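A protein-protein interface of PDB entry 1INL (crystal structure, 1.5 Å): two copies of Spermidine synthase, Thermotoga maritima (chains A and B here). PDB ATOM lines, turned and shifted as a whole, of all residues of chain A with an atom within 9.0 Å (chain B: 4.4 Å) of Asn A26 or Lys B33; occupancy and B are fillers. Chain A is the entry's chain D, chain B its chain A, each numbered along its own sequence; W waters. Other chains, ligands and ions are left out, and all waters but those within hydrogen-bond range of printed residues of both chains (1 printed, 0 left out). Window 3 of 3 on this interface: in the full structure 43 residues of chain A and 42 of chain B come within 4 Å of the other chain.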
ATOM      1  N   PHE A  20       2.505   7.823  -7.340  1.00  0.00           N
ATOM      2  CA  PHE A  20       3.895   7.721  -6.890  1.00  0.00           C
ATOM      3  C   PHE A  20       3.943   8.037  -5.399  1.00  0.00           C
ATOM      4  O   PHE A  20       3.554   9.132  -4.985  1.00  0.00           O
ATOM      5  CB  PHE A  20       4.797   8.747  -7.600  1.00  0.00           C
ATOM      6  CG  PHE A  20       5.119   8.428  -9.037  1.00  0.00           C
ATOM      7  CD1 PHE A  20       4.556   7.337  -9.690  1.00  0.00           C
ATOM      8  CD2 PHE A  20       5.992   9.249  -9.743  1.00  0.00           C
ATOM      9  CE1 PHE A  20       4.860   7.070 -11.026  1.00  0.00           C
ATOM     10  CE2 PHE A  20       6.302   8.990 -11.076  1.00  0.00           C
ATOM     11  CZ  PHE A  20       5.732   7.897 -11.718  1.00  0.00           C
ATOM     12  N   GLU A  21       4.413   7.082  -4.598  1.00  0.00           N
ATOM     13  CA  GLU A  21       4.554   7.280  -3.157  1.00  0.00           C
ATOM     14  C   GLU A  21       6.040   7.370  -2.817  1.00  0.00           C
ATOM     15  O   GLU A  21       6.779   6.402  -2.990  1.00  0.00           O
ATOM     16  CB  GLU A  21       3.937   6.124  -2.369  1.00  0.00           C
ATOM     17  CG  GLU A  21       4.158   6.265  -0.858  1.00  0.00           C
ATOM     18  CD  GLU A  21       3.771   5.037  -0.049  1.00  0.00           C
ATOM     19  OE1 GLU A  21       3.678   3.925  -0.614  1.00  0.00           O
ATOM     20  OE2 GLU A  21       3.581   5.185   1.176  1.00  0.00           O
ATOM     21  N   TYR A  22       6.478   8.532  -2.351  1.00  0.00           N
ATOM     22  CA  TYR A  22       7.876   8.717  -1.982  1.00  0.00           C
ATOM     23  C   TYR A  22       8.108   8.324  -0.527  1.00  0.00           C
ATOM     24  O   TYR A  22       7.297   8.635   0.345  1.00  0.00           O
ATOM     25  CB  TYR A  22       8.301  10.174  -2.206  1.00  0.00           C
ATOM     26  CG  TYR A  22       8.322  10.584  -3.660  1.00  0.00           C
ATOM     27  CD1 TYR A  22       7.151  10.961  -4.320  1.00  0.00           C
ATOM     28  CD2 TYR A  22       9.512  10.571  -4.389  1.00  0.00           C
ATOM     29  CE1 TYR A  22       7.163  11.312  -5.668  1.00  0.00           C
ATOM     30  CE2 TYR A  22       9.534  10.920  -5.736  1.00  0.00           C
ATOM     31  CZ  TYR A  22       8.358  11.287  -6.370  1.00  0.00           C
ATOM     32  OH  TYR A  22       8.377  11.624  -7.703  1.00  0.00           O
ATOM     33  N   TYR A  23       9.193   7.598  -0.276  1.00  0.00           N
ATOM     34  CA  TYR A  23       9.536   7.185   1.082  1.00  0.00           C
ATOM     35  C   TYR A  23      10.348   8.291   1.733  1.00  0.00           C
ATOM     36  O   TYR A  23      10.837   9.193   1.052  1.00  0.00           O
ATOM     37  CB  TYR A  23      10.368   5.901   1.071  1.00  0.00           C
ATOM     38  CG  TYR A  23       9.668   4.706   0.476  1.00  0.00           C
ATOM     39  CD1 TYR A  23       8.275   4.642   0.410  1.00  0.00           C
ATOM     40  CD2 TYR A  23      10.399   3.627  -0.010  1.00  0.00           C
ATOM     41  CE1 TYR A  23       7.632   3.532  -0.122  1.00  0.00           C
ATOM     42  CE2 TYR A  23       9.770   2.512  -0.541  1.00  0.00           C
ATOM     43  CZ  TYR A  23       8.388   2.470  -0.594  1.00  0.00           C
ATOM     44  OH  TYR A  23       7.770   1.361  -1.116  1.00  0.00           O
ATOM     45  N   THR A  24      10.493   8.218   3.053  1.00  0.00           N
ATOM     46  CA  THR A  24      11.260   9.214   3.789  1.00  0.00           C
ATOM     47  C   THR A  24      12.645   9.350   3.160  1.00  0.00           C
ATOM     48  O   THR A  24      13.339   8.356   2.942  1.00  0.00           O
ATOM     49  CB  THR A  24      11.371   8.823   5.269  1.00  0.00           C
ATOM     50  OG1 THR A  24      10.058   8.805   5.837  1.00  0.00           O
ATOM     51  CG2 THR A  24      12.245   9.818   6.040  1.00  0.00           C
ATOM     52  N   GLY A  25      13.008  10.580   2.814  1.00  0.00           N
ATOM     53  CA  GLY A  25      14.292  10.831   2.182  1.00  0.00           C
ATOM     54  C   GLY A  25      14.117  11.193   0.719  1.00  0.00           C
ATOM     55  O   GLY A  25      14.988  11.825   0.117  1.00  0.00           O
ATOM     56  N   ASN A  26      12.989  10.774   0.144  1.00  0.00           N
ATOM     57  CA  ASN A  26      12.642  11.049  -1.252  1.00  0.00           C
ATOM     58  C   ASN A  26      13.606  10.475  -2.288  1.00  0.00           C
ATOM     59  O   ASN A  26      13.701  10.985  -3.406  1.00  0.00           O
ATOM     60  CB  ASN A  26      12.480  12.558  -1.470  1.00  0.00           C
ATOM     61  CG  ASN A  26      11.429  13.165  -0.564  1.00  0.00           C
ATOM     62  OD1 ASN A  26      10.365  12.584  -0.357  1.00  0.00           O
ATOM     63  ND2 ASN A  26      11.725  14.337  -0.012  1.00  0.00           N
ATOM     64  N   ASN A  27      14.283   9.389  -1.928  1.00  0.00           N
ATOM     65  CA  ASN A  27      15.242   8.747  -2.824  1.00  0.00           C
ATOM     66  C   ASN A  27      14.745   7.416  -3.374  1.00  0.00           C
ATOM     67  O   ASN A  27      15.310   6.883  -4.334  1.00  0.00           O
ATOM     68  CB  ASN A  27      16.569   8.528  -2.106  1.00  0.00           C
ATOM     69  CG  ASN A  27      17.238   9.826  -1.721  1.00  0.00           C
ATOM     70  OD1 ASN A  27      17.466  10.687  -2.566  1.00  0.00           O
ATOM     71  ND2 ASN A  27      17.550   9.975  -0.442  1.00  0.00           N
ATOM     72  N   VAL A  28      13.714   6.870  -2.735  1.00  0.00           N
ATOM     73  CA  VAL A  28      13.118   5.596  -3.126  1.00  0.00           C
ATOM     74  C   VAL A  28      11.612   5.726  -2.919  1.00  0.00           C
ATOM     75  O   VAL A  28      11.161   6.530  -2.099  1.00  0.00           O
ATOM     76  CB  VAL A  28      13.637   4.416  -2.237  1.00  0.00           C
ATOM     77  CG1 VAL A  28      13.090   3.084  -2.735  1.00  0.00           C
ATOM     78  CG2 VAL A  28      15.156   4.369  -2.224  1.00  0.00           C
ATOM     79  N   GLY A  29      10.838   4.961  -3.681  1.00  0.00           N
ATOM     80  CA  GLY A  29       9.396   5.007  -3.528  1.00  0.00           C
ATOM     81  C   GLY A  29       8.701   3.872  -4.246  1.00  0.00           C
ATOM     82  O   GLY A  29       9.341   3.056  -4.907  1.00  0.00           O
ATOM     83  N   GLY A  64      -0.369  11.562  -0.099  1.00  0.00           N
ATOM     84  CA  GLY A  64       0.530  10.775  -0.929  1.00  0.00           C
ATOM     85  C   GLY A  64       1.255   9.636  -0.238  1.00  0.00           C
ATOM     86  O   GLY A  64       2.277   9.162  -0.739  1.00  0.00           O
ATOM     87  N   ILE A  65       0.756   9.222   0.924  1.00  0.00           N
ATOM     88  CA  ILE A  65       1.345   8.118   1.678  1.00  0.00           C
ATOM     89  C   ILE A  65       0.286   7.023   1.760  1.00  0.00           C
ATOM     90  O   ILE A  65      -0.847   7.283   2.159  1.00  0.00           O
ATOM     91  CB  ILE A  65       1.743   8.553   3.110  1.00  0.00           C
ATOM     92  CG1 ILE A  65       2.788   9.670   3.048  1.00  0.00           C
ATOM     93  CG2 ILE A  65       2.286   7.358   3.898  1.00  0.00           C
ATOM     94  CD1 ILE A  65       3.179  10.225   4.403  1.00  0.00           C
ATOM     95  N   TYR A 210      13.811   2.980   6.360  1.00  0.00           N
ATOM     96  CA  TYR A 210      13.719   4.372   5.911  1.00  0.00           C
ATOM     97  C   TYR A 210      13.345   5.296   7.063  1.00  0.00           C
ATOM     98  O   TYR A 210      13.704   6.476   7.071  1.00  0.00           O
ATOM     99  CB  TYR A 210      12.664   4.523   4.809  1.00  0.00           C
ATOM    100  CG  TYR A 210      12.970   3.745   3.556  1.00  0.00           C
ATOM    101  CD1 TYR A 210      14.039   4.102   2.734  1.00  0.00           C
ATOM    102  CD2 TYR A 210      12.209   2.630   3.206  1.00  0.00           C
ATOM    103  CE1 TYR A 210      14.347   3.363   1.600  1.00  0.00           C
ATOM    104  CE2 TYR A 210      12.506   1.886   2.072  1.00  0.00           C
ATOM    105  CZ  TYR A 210      13.580   2.256   1.277  1.00  0.00           C
ATOM    106  OH  TYR A 210      13.908   1.499   0.177  1.00  0.00           O
ATOM    107  N   PRO B  13      23.058  14.374  -6.047  1.00  0.00           N
ATOM    108  CA  PRO B  13      21.804  13.859  -6.607  1.00  0.00           C
ATOM    109  C   PRO B  13      20.749  14.926  -6.848  1.00  0.00           C
ATOM    110  O   PRO B  13      20.633  15.889  -6.083  1.00  0.00           O
ATOM    111  CB  PRO B  13      21.322  12.875  -5.534  1.00  0.00           C
ATOM    112  CG  PRO B  13      22.541  12.576  -4.720  1.00  0.00           C
ATOM    113  CD  PRO B  13      23.244  13.888  -4.671  1.00  0.00           C
ATOM    114  N   ARG B  14      19.989  14.756  -7.926  1.00  0.00           N
ATOM    115  CA  ARG B  14      18.911  15.676  -8.266  1.00  0.00           C
ATOM    116  C   ARG B  14      17.648  14.843  -8.488  1.00  0.00           C
ATOM    117  O   ARG B  14      17.598  13.686  -8.072  1.00  0.00           O
ATOM    118  CB  ARG B  14      19.267  16.523  -9.491  1.00  0.00           C
ATOM    119  CG  ARG B  14      20.502  17.400  -9.288  1.00  0.00           C
ATOM    120  CD  ARG B  14      20.690  18.407 -10.418  1.00  0.00           C
ATOM    121  NE  ARG B  14      19.726  19.504 -10.358  1.00  0.00           N
ATOM    122  CZ  ARG B  14      19.914  20.635  -9.681  1.00  0.00           C
ATOM    123  NH1 ARG B  14      21.034  20.831  -8.997  1.00  0.00           N
ATOM    124  NH2 ARG B  14      18.982  21.581  -9.698  1.00  0.00           N
ATOM    125  N   LEU B  17      17.180  11.684 -12.700  1.00  0.00           N
ATOM    126  CA  LEU B  17      17.560  10.329 -13.117  1.00  0.00           C
ATOM    127  C   LEU B  17      16.880   9.292 -12.246  1.00  0.00           C
ATOM    128  O   LEU B  17      17.017   9.320 -11.021  1.00  0.00           O
ATOM    129  CB  LEU B  17      19.076  10.146 -13.054  1.00  0.00           C
ATOM    130  CG  LEU B  17      19.934  11.126 -13.862  1.00  0.00           C
ATOM    131  CD1 LEU B  17      21.395  10.750 -13.690  1.00  0.00           C
ATOM    132  CD2 LEU B  17      19.547  11.114 -15.341  1.00  0.00           C
ATOM    133  N   TRP B  18      16.184   8.352 -12.885  1.00  0.00           N
ATOM    134  CA  TRP B  18      15.434   7.334 -12.163  1.00  0.00           C
ATOM    135  C   TRP B  18      15.520   5.923 -12.715  1.00  0.00           C
ATOM    136  O   TRP B  18      15.689   5.708 -13.916  1.00  0.00           O
ATOM    137  CB  TRP B  18      13.952   7.725 -12.116  1.00  0.00           C
ATOM    138  CG  TRP B  18      13.711   9.058 -11.503  1.00  0.00           C
ATOM    139  CD1 TRP B  18      13.681  10.261 -12.147  1.00  0.00           C
ATOM    140  CD2 TRP B  18      13.532   9.339 -10.111  1.00  0.00           C
ATOM    141  NE1 TRP B  18      13.507  11.278 -11.239  1.00  0.00           N
ATOM    142  CE2 TRP B  18      13.412  10.740  -9.982  1.00  0.00           C
ATOM    143  CE3 TRP B  18      13.464   8.545  -8.958  1.00  0.00           C
ATOM    144  CZ2 TRP B  18      13.229  11.366  -8.743  1.00  0.00           C
ATOM    145  CZ3 TRP B  18      13.281   9.168  -7.725  1.00  0.00           C
ATOM    146  CH2 TRP B  18      13.167  10.567  -7.631  1.00  0.00           C
ATOM    147  N   MET B  32      13.754   4.249  -7.891  1.00  0.00           N
ATOM    148  CA  MET B  32      14.919   4.713  -7.142  1.00  0.00           C
ATOM    149  C   MET B  32      15.622   5.845  -7.869  1.00  0.00           C
ATOM    150  O   MET B  32      15.791   5.807  -9.089  1.00  0.00           O
ATOM    151  CB  MET B  32      15.949   3.586  -6.981  1.00  0.00           C
ATOM    152  CG  MET B  32      15.497   2.344  -6.241  1.00  0.00           C
ATOM    153  SD  MET B  32      16.880   1.178  -6.216  1.00  0.00           S
ATOM    154  CE  MET B  32      16.068  -0.305  -5.691  1.00  0.00           C
ATOM    155  N   LYS B  33      16.068   6.834  -7.105  1.00  0.00           N
ATOM    156  CA  LYS B  33      16.811   7.957  -7.653  1.00  0.00           C
ATOM    157  C   LYS B  33      18.224   7.439  -7.956  1.00  0.00           C
ATOM    158  O   LYS B  33      18.753   6.597  -7.226  1.00  0.00           O
ATOM    159  CB  LYS B  33      16.875   9.076  -6.608  1.00  0.00           C
ATOM    160  CG  LYS B  33      17.638  10.316  -7.033  1.00  0.00           C
ATOM    161  CD  LYS B  33      17.608  11.378  -5.936  1.00  0.00           C
ATOM    162  CE  LYS B  33      16.190  11.876  -5.687  1.00  0.00           C
ATOM    163  NZ  LYS B  33      16.131  12.910  -4.617  1.00  0.00           N
ATOM    164  N   MET B  34      18.796   7.868  -9.076  1.00  0.00           N
ATOM    165  CA  MET B  34      20.151   7.449  -9.424  1.00  0.00           C
ATOM    166  C   MET B  34      21.084   8.646  -9.390  1.00  0.00           C
ATOM    167  O   MET B  34      20.887   9.606 -10.138  1.00  0.00           O
ATOM    168  CB  MET B  34      20.209   6.837 -10.826  1.00  0.00           C
ATOM    169  CG  MET B  34      19.279   5.671 -11.048  1.00  0.00           C
ATOM    170  SD  MET B  34      19.698   4.728 -12.535  1.00  0.00           S
ATOM    171  CE  MET B  34      19.233   5.891 -13.818  1.00  0.00           C
ATOM    172  N   ASN B  35      22.080   8.615  -8.509  1.00  0.00           N
ATOM    173  CA  ASN B  35      23.037   9.716  -8.470  1.00  0.00           C
ATOM    174  C   ASN B  35      23.980   9.558  -9.656  1.00  0.00           C
ATOM    175  O   ASN B  35      24.415  10.539 -10.248  1.00  0.00           O
ATOM    176  CB  ASN B  35      23.844   9.735  -7.175  1.00  0.00           C
ATOM    177  CG  ASN B  35      24.703  10.976  -7.064  1.00  0.00           C
ATOM    178  OD1 ASN B  35      24.288  12.059  -7.476  1.00  0.00           O
ATOM    179  ND2 ASN B  35      25.914  10.824  -6.542  1.00  0.00           N
ATOM    180  N   PHE B  51      24.241   0.948 -10.379  1.00  0.00           N
ATOM    181  CA  PHE B  51      24.173   2.389 -10.164  1.00  0.00           C
ATOM    182  C   PHE B  51      24.206   2.732  -8.685  1.00  0.00           C
ATOM    183  O   PHE B  51      24.199   1.847  -7.839  1.00  0.00           O
ATOM    184  CB  PHE B  51      22.917   2.972 -10.839  1.00  0.00           C
ATOM    185  CG  PHE B  51      21.622   2.458 -10.272  1.00  0.00           C
ATOM    186  CD1 PHE B  51      21.035   1.302 -10.779  1.00  0.00           C
ATOM    187  CD2 PHE B  51      20.992   3.130  -9.227  1.00  0.00           C
ATOM    188  CE1 PHE B  51      19.836   0.822 -10.251  1.00  0.00           C
ATOM    189  CE2 PHE B  51      19.797   2.661  -8.692  1.00  0.00           C
ATOM    190  CZ  PHE B  51      19.218   1.502  -9.208  1.00  0.00           C
ATOM    191  N   GLU B  52      24.249   4.027  -8.385  1.00  0.00           N
ATOM    192  CA  GLU B  52      24.313   4.507  -7.012  1.00  0.00           C
ATOM    193  C   GLU B  52      23.050   5.257  -6.602  1.00  0.00           C
ATOM    194  O   GLU B  52      22.607   6.164  -7.302  1.00  0.00           O
ATOM    195  CB  GLU B  52      25.533   5.419  -6.881  1.00  0.00           C
ATOM    196  CG  GLU B  52      25.765   6.057  -5.527  1.00  0.00           C
ATOM    197  CD  GLU B  52      26.852   7.117  -5.590  1.00  0.00           C
ATOM    198  OE1 GLU B  52      26.559   8.290  -5.282  1.00  0.00           O
ATOM    199  OE2 GLU B  52      27.996   6.781  -5.972  1.00  0.00           O
ATOM    200  N   ASN B  53      22.457   4.841  -5.485  1.00  0.00           N
ATOM    201  CA  ASN B  53      21.262   5.483  -4.929  1.00  0.00           C
ATOM    202  C   ASN B  53      21.697   6.121  -3.608  1.00  0.00           C
ATOM    203  O   ASN B  53      22.421   5.506  -2.828  1.00  0.00           O
ATOM    204  CB  ASN B  53      20.152   4.456  -4.669  1.00  0.00           C
ATOM    205  CG  ASN B  53      18.952   5.059  -3.947  1.00  0.00           C
ATOM    206  OD1 ASN B  53      18.850   4.984  -2.724  1.00  0.00           O
ATOM    207  ND2 ASN B  53      18.044   5.665  -4.702  1.00  0.00           N
ATOM    208  N   PRO B  54      21.256   7.361  -3.339  1.00  0.00           N
ATOM    209  CA  PRO B  54      21.617   8.068  -2.105  1.00  0.00           C
ATOM    210  C   PRO B  54      21.367   7.315  -0.797  1.00  0.00           C
ATOM    211  O   PRO B  54      22.163   7.418   0.137  1.00  0.00           O
ATOM    212  CB  PRO B  54      20.780   9.339  -2.194  1.00  0.00           C
ATOM    213  CG  PRO B  54      20.777   9.615  -3.659  1.00  0.00           C
ATOM    214  CD  PRO B  54      20.494   8.246  -4.241  1.00  0.00           C
HETATM  215  O   HOH W   1      18.897  12.957  -2.657  1.00  0.00           O
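Among the printed residues, pairs that only touch across the chains: Asn A27 with Met B32 (3.6 Å), Asn A27 with Pro B54 (3.6 Å) and Val A28 with Asn B53 (3.8 Å).
O of Asn A26 is in hydrogen-bond range of NZ of Lys B33 (3.3 Å).
The side-chain amide nitrogen (ND2) of Asn B53 lies within hydrogen-bond range of the backbone carbonyl oxygen (O) of Asn A27, 3.0 Å away.
The backbone carbonyl oxygen of Asn A27 sits at hydrogen-bond distance from the backbone NH of Lys B33 (2.9 Å).
No position is printed for both chains.
O of Val A28 is in hydrogen-bond range of N of Tyr A23.
The backbone carbonyl oxygen (O) of Lys B33 sits at hydrogen-bond distance from the side-chain amide nitrogen (ND2) of Asn B53 (2.8 Å).
The side-chain amide nitrogen of Asn A27 sits at hydrogen-bond distance from the backbone carbonyl oxygen of Gly A25, 3.2 Å away.
Water W1 lies within hydrogen-bond range of the side-chain amide oxygen of Asn A27 (2.7 Å) and the side-chain amino group of Lys B33 (3.4 Å).
Gly A25 touches none of the printed residues of chain B.
Of the printed residues of chain B, Val A28 touches Asn B53 (3.8 Å).
Printed residues of chain A within 4 Å of Met B32: Asn A27 (3.6 Å).
Of chain A, only Asn A26 (3.3 Å) and Asn A27 (2.9 Å) come within 4 Å of Lys B33.
Of the printed residues of chain A, Asn B53 touches Asn A27 (3.0 Å) and Val A28 (3.8 Å).
The nearest residue of chain B that does not touch Asn A26 is Trp B18 (4.3 Å).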
